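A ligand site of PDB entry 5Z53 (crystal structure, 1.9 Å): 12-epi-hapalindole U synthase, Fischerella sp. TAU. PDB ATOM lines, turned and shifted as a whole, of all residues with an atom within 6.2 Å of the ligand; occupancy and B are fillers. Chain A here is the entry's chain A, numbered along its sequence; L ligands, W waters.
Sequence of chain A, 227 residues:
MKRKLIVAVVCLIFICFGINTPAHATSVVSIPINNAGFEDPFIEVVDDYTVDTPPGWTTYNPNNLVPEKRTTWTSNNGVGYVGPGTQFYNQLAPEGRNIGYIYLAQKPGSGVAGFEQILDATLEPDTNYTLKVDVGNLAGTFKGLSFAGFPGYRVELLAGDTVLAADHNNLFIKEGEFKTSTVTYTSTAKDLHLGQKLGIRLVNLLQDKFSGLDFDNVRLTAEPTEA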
ATOM      1  N   VAL A  46       1.618  -7.313  -1.141  1.00  0.00           N
ATOM      2  CA  VAL A  46       1.583  -8.672  -0.628  1.00  0.00           C
ATOM      3  C   VAL A  46       2.648  -8.825   0.463  1.00  0.00           C
ATOM      4  O   VAL A  46       3.795  -8.321   0.323  1.00  0.00           O
ATOM      5  CB  VAL A  46       1.799  -9.721  -1.724  1.00  0.00           C
ATOM      6  CG1 VAL A  46       3.188  -9.603  -2.338  1.00  0.00           C
ATOM      7  CG2 VAL A  46       1.586 -11.108  -1.181  1.00  0.00           C
ATOM      8  N   ASP A  47       2.253  -9.496   1.543  1.00  0.00           N
ATOM      9  CA  ASP A  47       3.046  -9.763   2.743  1.00  0.00           C
ATOM     10  C   ASP A  47       3.300  -8.511   3.594  1.00  0.00           C
ATOM     11  O   ASP A  47       3.976  -8.616   4.632  1.00  0.00           O
ATOM     12  CB  ASP A  47       4.347 -10.492   2.414  1.00  0.00           C
ATOM     13  CG  ASP A  47       4.125 -11.920   1.945  1.00  0.00           C
ATOM     14  OD1 ASP A  47       3.155 -12.549   2.418  1.00  0.00           O
ATOM     15  OD2 ASP A  47       4.950 -12.422   1.131  1.00  0.00           O
ATOM     16  N   ASP A  48       2.771  -7.339   3.219  1.00  0.00           N
ATOM     17  CA  ASP A  48       2.872  -6.198   4.126  1.00  0.00           C
ATOM     18  C   ASP A  48       1.866  -6.368   5.280  1.00  0.00           C
ATOM     19  O   ASP A  48       0.932  -7.179   5.254  1.00  0.00           O
ATOM     20  CB  ASP A  48       2.651  -4.878   3.376  1.00  0.00           C
ATOM     21  CG  ASP A  48       3.042  -3.658   4.182  1.00  0.00           C
ATOM     22  OD1 ASP A  48       3.868  -3.789   5.120  1.00  0.00           O
ATOM     23  OD2 ASP A  48       2.517  -2.607   3.882  1.00  0.00           O
ATOM     24  N   TYR A  49       2.028  -5.567   6.348  1.00  0.00           N
ATOM     25  CA  TYR A  49       1.266  -5.752   7.533  1.00  0.00           C
ATOM     26  C   TYR A  49       1.314  -4.466   8.364  1.00  0.00           C
ATOM     27  O   TYR A  49       2.253  -3.690   8.227  1.00  0.00           O
ATOM     28  CB  TYR A  49       1.845  -6.911   8.352  1.00  0.00           C
ATOM     29  CG  TYR A  49       3.273  -6.708   8.812  1.00  0.00           C
ATOM     30  CD1 TYR A  49       4.356  -7.020   8.003  1.00  0.00           C
ATOM     31  CD2 TYR A  49       3.546  -6.280  10.091  1.00  0.00           C
ATOM     32  CE1 TYR A  49       5.679  -6.959   8.454  1.00  0.00           C
ATOM     33  CE2 TYR A  49       4.852  -6.142  10.539  1.00  0.00           C
ATOM     34  CZ  TYR A  49       5.917  -6.468   9.732  1.00  0.00           C
ATOM     35  OH  TYR A  49       7.209  -6.343  10.168  1.00  0.00           O
ATOM     36  N   VAL A  79      -2.923  -6.445  11.004  1.00  0.00           N
ATOM     37  CA  VAL A  79      -3.443  -7.225   9.858  1.00  0.00           C
ATOM     38  C   VAL A  79      -2.284  -7.447   8.894  1.00  0.00           C
ATOM     39  O   VAL A  79      -1.277  -6.723   8.869  1.00  0.00           O
ATOM     40  CB  VAL A  79      -4.638  -6.561   9.148  1.00  0.00           C
ATOM     41  CG1 VAL A  79      -5.748  -6.205  10.137  1.00  0.00           C
ATOM     42  CG2 VAL A  79      -4.234  -5.351   8.331  1.00  0.00           C
ATOM     43  N   GLY A  80      -2.442  -8.449   8.032  1.00  0.00           N
ATOM     44  CA  GLY A  80      -1.399  -8.754   7.084  1.00  0.00           C
ATOM     45  C   GLY A  80      -2.039  -9.280   5.806  1.00  0.00           C
ATOM     46  O   GLY A  80      -3.055  -9.964   5.936  1.00  0.00           O
ATOM     47  N   TYR A  81      -1.434  -8.962   4.665  1.00  0.00           N
ATOM     48  CA  TYR A  81      -2.031  -9.284   3.360  1.00  0.00           C
ATOM     49  C   TYR A  81      -1.442 -10.618   2.923  1.00  0.00           C
ATOM     50  O   TYR A  81      -0.256 -10.719   2.670  1.00  0.00           O
ATOM     51  CB  TYR A  81      -1.771  -8.156   2.370  1.00  0.00           C
ATOM     52  CG  TYR A  81      -2.203  -8.378   0.938  1.00  0.00           C
ATOM     53  CD1 TYR A  81      -3.229  -9.215   0.575  1.00  0.00           C
ATOM     54  CD2 TYR A  81      -1.578  -7.665  -0.070  1.00  0.00           C
ATOM     55  CE1 TYR A  81      -3.606  -9.357  -0.763  1.00  0.00           C
ATOM     56  CE2 TYR A  81      -1.934  -7.788  -1.402  1.00  0.00           C
ATOM     57  CZ  TYR A  81      -2.941  -8.661  -1.757  1.00  0.00           C
ATOM     58  OH  TYR A  81      -3.209  -8.816  -3.102  1.00  0.00           O
ATOM     59  N   VAL A  82      -2.314 -11.629   2.854  1.00  0.00           N
ATOM     60  CA  VAL A  82      -1.867 -12.927   2.404  1.00  0.00           C
ATOM     61  C   VAL A  82      -2.443 -13.083   1.004  1.00  0.00           C
ATOM     62  O   VAL A  82      -3.520 -13.608   0.830  1.00  0.00           O
ATOM     63  CB  VAL A  82      -2.290 -14.078   3.332  1.00  0.00           C
ATOM     64  CG1 VAL A  82      -1.745 -15.405   2.806  1.00  0.00           C
ATOM     65  CG2 VAL A  82      -1.789 -13.813   4.762  1.00  0.00           C
ATOM     66  N   THR A  86       2.527 -14.732  -2.033  1.00  0.00           N
ATOM     67  CA  THR A  86       3.034 -14.635  -0.648  1.00  0.00           C
ATOM     68  C   THR A  86       4.232 -15.583  -0.542  1.00  0.00           C
ATOM     69  O   THR A  86       4.211 -16.620  -1.165  1.00  0.00           O
ATOM     70  CB  THR A  86       1.987 -14.963   0.430  1.00  0.00           C
ATOM     71  OG1 THR A  86       2.636 -15.097   1.692  1.00  0.00           O
ATOM     72  CG2 THR A  86       1.198 -16.234   0.170  1.00  0.00           C
ATOM     73  N   GLN A  87       5.236 -15.249   0.266  1.00  0.00           N
ATOM     74  CA  GLN A  87       6.402 -16.117   0.409  1.00  0.00           C
ATOM     75  C   GLN A  87       6.244 -17.035   1.626  1.00  0.00           C
ATOM     76  O   GLN A  87       7.084 -17.921   1.846  1.00  0.00           O
ATOM     77  CB  GLN A  87       7.703 -15.322   0.626  1.00  0.00           C
ATOM     78  CG  GLN A  87       8.258 -14.525  -0.543  1.00  0.00           C
ATOM     79  CD  GLN A  87       9.325 -13.597   0.021  1.00  0.00           C
ATOM     80  OE1 GLN A  87      10.342 -14.019   0.571  1.00  0.00           O
ATOM     81  NE2 GLN A  87       9.074 -12.296  -0.038  1.00  0.00           N
ATOM     82  N   PHE A  88       5.161 -16.884   2.388  1.00  0.00           N
ATOM     83  CA  PHE A  88       5.079 -17.442   3.718  1.00  0.00           C
ATOM     84  C   PHE A  88       3.917 -18.423   3.936  1.00  0.00           C
ATOM     85  O   PHE A  88       3.761 -18.957   5.039  1.00  0.00           O
ATOM     86  CB  PHE A  88       5.086 -16.280   4.715  1.00  0.00           C
ATOM     87  CG  PHE A  88       6.244 -15.329   4.500  1.00  0.00           C
ATOM     88  CD1 PHE A  88       7.565 -15.757   4.593  1.00  0.00           C
ATOM     89  CD2 PHE A  88       6.025 -13.998   4.167  1.00  0.00           C
ATOM     90  CE1 PHE A  88       8.623 -14.889   4.376  1.00  0.00           C
ATOM     91  CE2 PHE A  88       7.087 -13.124   3.981  1.00  0.00           C
ATOM     92  CZ  PHE A  88       8.393 -13.580   4.046  1.00  0.00           C
ATOM     93  N   TYR A  89       3.146 -18.739   2.891  1.00  0.00           N
ATOM     94  CA  TYR A  89       2.021 -19.646   3.001  1.00  0.00           C
ATOM     95  C   TYR A  89       1.925 -20.437   1.701  1.00  0.00           C
ATOM     96  O   TYR A  89       2.446 -19.984   0.664  1.00  0.00           O
ATOM     97  CB  TYR A  89       0.703 -18.863   3.208  1.00  0.00           C
ATOM     98  CG  TYR A  89       0.424 -18.478   4.650  1.00  0.00           C
ATOM     99  CD1 TYR A  89      -0.059 -19.422   5.535  1.00  0.00           C
ATOM    100  CD2 TYR A  89       0.671 -17.197   5.138  1.00  0.00           C
ATOM    101  CE1 TYR A  89      -0.316 -19.108   6.858  1.00  0.00           C
ATOM    102  CE2 TYR A  89       0.417 -16.879   6.470  1.00  0.00           C
ATOM    103  CZ  TYR A  89      -0.083 -17.827   7.329  1.00  0.00           C
ATOM    104  OH  TYR A  89      -0.323 -17.589   8.655  1.00  0.00           O
ATOM    105  N   ILE A  99      -5.425 -11.281   6.881  1.00  0.00           N
ATOM    106  CA  ILE A  99      -5.587 -11.951   8.129  1.00  0.00           C
ATOM    107  C   ILE A  99      -5.306 -10.965   9.287  1.00  0.00           C
ATOM    108  O   ILE A  99      -4.793  -9.860   9.081  1.00  0.00           O
ATOM    109  CB  ILE A  99      -4.685 -13.195   8.130  1.00  0.00           C
ATOM    110  CG1 ILE A  99      -3.180 -12.930   7.965  1.00  0.00           C
ATOM    111  CG2 ILE A  99      -5.146 -14.097   6.977  1.00  0.00           C
ATOM    112  CD1 ILE A  99      -2.461 -12.293   9.149  1.00  0.00           C
ATOM    113  N   GLY A 100      -5.629 -11.394  10.510  1.00  0.00           N
ATOM    114  CA  GLY A 100      -5.167 -10.692  11.751  1.00  0.00           C
ATOM    115  C   GLY A 100      -4.090 -11.540  12.394  1.00  0.00           C
ATOM    116  O   GLY A 100      -4.258 -12.764  12.563  1.00  0.00           O
ATOM    117  N   TYR A 101      -3.009 -10.898  12.843  1.00  0.00           N
ATOM    118  CA  TYR A 101      -1.904 -11.660  13.436  1.00  0.00           C
ATOM    119  C   TYR A 101      -1.590 -11.097  14.826  1.00  0.00           C
ATOM    120  O   TYR A 101      -1.845  -9.917  15.081  1.00  0.00           O
ATOM    121  CB  TYR A 101      -0.665 -11.598  12.570  1.00  0.00           C
ATOM    122  CG  TYR A 101       0.105 -10.303  12.676  1.00  0.00           C
ATOM    123  CD1 TYR A 101       1.043 -10.140  13.669  1.00  0.00           C
ATOM    124  CD2 TYR A 101      -0.218  -9.186  11.918  1.00  0.00           C
ATOM    125  CE1 TYR A 101       1.653  -8.917  13.898  1.00  0.00           C
ATOM    126  CE2 TYR A 101       0.405  -7.955  12.115  1.00  0.00           C
ATOM    127  CZ  TYR A 101       1.336  -7.823  13.125  1.00  0.00           C
ATOM    128  OH  TYR A 101       1.932  -6.634  13.399  1.00  0.00           O
ATOM    129  N   LEU A 138       2.363 -19.326   9.895  1.00  0.00           N
ATOM    130  CA  LEU A 138       3.365 -18.667   8.995  1.00  0.00           C
ATOM    131  C   LEU A 138       4.526 -19.623   8.757  1.00  0.00           C
ATOM    132  O   LEU A 138       5.011 -20.234   9.713  1.00  0.00           O
ATOM    133  CB  LEU A 138       3.968 -17.450   9.689  1.00  0.00           C
ATOM    134  CG  LEU A 138       3.870 -16.040   9.093  1.00  0.00           C
ATOM    135  CD1 LEU A 138       5.179 -15.329   9.331  1.00  0.00           C
ATOM    136  CD2 LEU A 138       3.505 -15.947   7.621  1.00  0.00           C
ATOM    137  N   PHE A 142      13.415 -15.627   6.160  1.00  0.00           N
ATOM    138  CA  PHE A 142      13.768 -14.418   5.506  1.00  0.00           C
ATOM    139  C   PHE A 142      15.084 -13.897   6.062  1.00  0.00           C
ATOM    140  O   PHE A 142      15.122 -13.418   7.184  1.00  0.00           O
ATOM    141  CB  PHE A 142      12.652 -13.412   5.739  1.00  0.00           C
ATOM    142  CG  PHE A 142      12.796 -12.188   4.886  1.00  0.00           C
ATOM    143  CD1 PHE A 142      12.299 -12.164   3.596  1.00  0.00           C
ATOM    144  CD2 PHE A 142      13.431 -11.063   5.395  1.00  0.00           C
ATOM    145  CE1 PHE A 142      12.427 -11.025   2.812  1.00  0.00           C
ATOM    146  CE2 PHE A 142      13.572  -9.939   4.612  1.00  0.00           C
ATOM    147  CZ  PHE A 142      13.062  -9.913   3.326  1.00  0.00           C
ATOM    148  N   LEU A 145      16.056 -14.855   9.526  1.00  0.00           N
ATOM    149  CA  LEU A 145      14.832 -14.939  10.312  1.00  0.00           C
ATOM    150  C   LEU A 145      14.091 -16.228   9.980  1.00  0.00           C
ATOM    151  O   LEU A 145      13.957 -16.569   8.814  1.00  0.00           O
ATOM    152  CB  LEU A 145      13.943 -13.802   9.836  1.00  0.00           C
ATOM    153  CG  LEU A 145      13.694 -12.698  10.828  1.00  0.00           C
ATOM    154  CD1 LEU A 145      13.073 -11.529  10.082  1.00  0.00           C
ATOM    155  CD2 LEU A 145      12.791 -13.219  11.918  1.00  0.00           C
ATOM    156  N   PHE A 147      10.560 -18.613  10.406  1.00  0.00           N
ATOM    157  CA  PHE A 147       9.180 -18.740  10.832  1.00  0.00           C
ATOM    158  C   PHE A 147       8.815 -20.180  11.182  1.00  0.00           C
ATOM    159  O   PHE A 147       7.634 -20.481  11.423  1.00  0.00           O
ATOM    160  CB  PHE A 147       8.258 -18.232   9.744  1.00  0.00           C
ATOM    161  CG  PHE A 147       8.412 -16.766   9.473  1.00  0.00           C
ATOM    162  CD1 PHE A 147       8.514 -15.861  10.509  1.00  0.00           C
ATOM    163  CD2 PHE A 147       8.448 -16.297   8.168  1.00  0.00           C
ATOM    164  CE1 PHE A 147       8.595 -14.507  10.261  1.00  0.00           C
ATOM    165  CE2 PHE A 147       8.553 -14.936   7.918  1.00  0.00           C
ATOM    166  CZ  PHE A 147       8.624 -14.043   8.961  1.00  0.00           C
ATOM    167  N   LEU A 213       1.108 -15.985  15.157  1.00  0.00           N
ATOM    168  CA  LEU A 213       0.074 -16.778  14.484  1.00  0.00           C
ATOM    169  C   LEU A 213      -0.988 -15.834  13.898  1.00  0.00           C
ATOM    170  O   LEU A 213      -1.131 -14.666  14.287  1.00  0.00           O
ATOM    171  CB  LEU A 213      -0.492 -17.853  15.416  1.00  0.00           C
ATOM    172  CG  LEU A 213      -1.653 -17.441  16.320  1.00  0.00           C
ATOM    173  CD1 LEU A 213      -2.016 -18.553  17.287  1.00  0.00           C
ATOM    174  CD2 LEU A 213      -1.324 -16.187  17.079  1.00  0.00           C
ATOM    175  N   ASP A 214      -1.716 -16.370  12.920  1.00  0.00           N
ATOM    176  CA  ASP A 214      -2.676 -15.631  12.147  1.00  0.00           C
ATOM    177  C   ASP A 214      -4.091 -16.168  12.405  1.00  0.00           C
ATOM    178  O   ASP A 214      -4.290 -17.347  12.638  1.00  0.00           O
ATOM    179  CB  ASP A 214      -2.289 -15.759  10.661  1.00  0.00           C
ATOM    180  CG  ASP A 214      -0.988 -15.070  10.255  1.00  0.00           C
ATOM    181  OD1 ASP A 214      -0.461 -14.260  11.056  1.00  0.00           O
ATOM    182  OD2 ASP A 214      -0.522 -15.249   9.088  1.00  0.00           O
HETATM  183  N1  LIG L   1       8.205 -10.574   7.764  1.00  0.00           N
HETATM  184  C1  LIG L   1       8.467 -10.675   6.297  1.00  0.00           C
HETATM  185  C2  LIG L   1       9.810 -10.036   6.259  1.00  0.00           C
HETATM  186  C3  LIG L   1      10.388 -10.844   7.369  1.00  0.00           C
HETATM  187  C4  LIG L   1       9.468 -10.499   8.516  1.00  0.00           C
HETATM  188  C5  LIG L   1       7.542  -9.961   5.507  1.00  0.00           C
HETATM  189  O1  LIG L   1       7.782  -9.432   4.429  1.00  0.00           O
HETATM  190  N2  LIG L   1       6.298  -9.773   5.982  1.00  0.00           N
HETATM  191  C6  LIG L   1       5.888 -10.343   7.317  1.00  0.00           C
HETATM  192  C7  LIG L   1       6.993 -10.321   8.231  1.00  0.00           C
HETATM  193  O2  LIG L   1       6.823 -10.191   9.445  1.00  0.00           O
HETATM  194  C8  LIG L   1       5.270 -11.758   7.211  1.00  0.00           C
HETATM  195  C9  LIG L   1       3.905 -11.792   6.426  1.00  0.00           C
HETATM  196  C10 LIG L   1       2.784 -10.852   7.007  1.00  0.00           C
HETATM  197  N3  LIG L   1       2.395 -11.243   8.394  1.00  0.00           N
HETATM  198  C11 LIG L   1       1.608 -12.311   8.666  1.00  0.00           C
HETATM  199  N4  LIG L   1       1.008 -13.001   7.679  1.00  0.00           N
HETATM  200  N5  LIG L   1       1.362 -12.645   9.931  1.00  0.00           N
HETATM  201  O   HOH W   1       5.670 -11.051  12.556  1.00  0.00           O
HETATM  202  O   HOH W   2       3.851 -10.114  10.582  1.00  0.00           O
HETATM  203  O   HOH W   3       1.361 -12.370   4.531  1.00  0.00           O
HETATM  204  O   HOH W   4       3.404 -13.001  12.715  1.00  0.00           O
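Water W3 lies within hydrogen-bond range of the side-chain carboxylate of Asp 47 (2.8 Å), the backbone carbonyl oxygen of Tyr 81 (3.0 Å) and a nitrogen (N4) of the ligand (3.2 Å).
The backbone carbonyl oxygen of Asp 47 is in hydrogen-bond range of a nitrogen (N2) of the ligand, 2.9 Å away.
The side-chain carboxylate (OD1) of Asp 214 lies within salt-bridge range of a nitrogen (N5) of the ligand (2.7 Å).
The backbone NH of Ile 99 sits at hydrogen-bond distance from the backbone carbonyl oxygen of Gly 80 (2.9 Å).
N of Asp 47 sits at hydrogen-bond distance from O of Tyr 81 (3.0 Å).
N of Leu 138 lies within hydrogen-bond range of OH of Tyr 89.
The side-chain carboxylate (OD2) of Asp 47 sits at hydrogen-bond distance from the backbone NH (N) of Gln 87 (3.0 Å).
The side-chain carboxylate (OD1) of Asp 47 lies within hydrogen-bond range of the side-chain hydroxyl (OG1) of Thr 86, at 2.7 Å.
The backbone NH (N) of Phe 88 sits at hydrogen-bond distance from the side-chain hydroxyl (OG1) of Thr 86 (3.2 Å).
Tyr 49 touches the ligand.
Phe 88 touches the ligand (CE2 to C5, 3.5 Å).
Ile 99 touches the ligand (CD1 to N4, 3.8 Å).
Tyr 101 touches the ligand.
CD2 of Leu 138 touches N4 of the ligand, 3.9 Å away.
Phe 142 touches the ligand.
Leu 145 touches the ligand (CD1 to C3, 3.9 Å).
Phe 147 touches the ligand.
Hydrophobic or aromatic side chains within 4 Å of the ligand: Tyr 49, Phe 88, Ile 99, Tyr 101, Leu 138, Phe 142, Leu 145 and Phe 147.
Within 4 Å of the ligand: Asp 47, Tyr 49, Phe 88, Ile 99, Tyr 101, Leu 138, Phe 142, Leu 145, Phe 147 and Asp 214.
The nearest printed residue that does not touch the ligand is Tyr 89 (4.1 Å).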
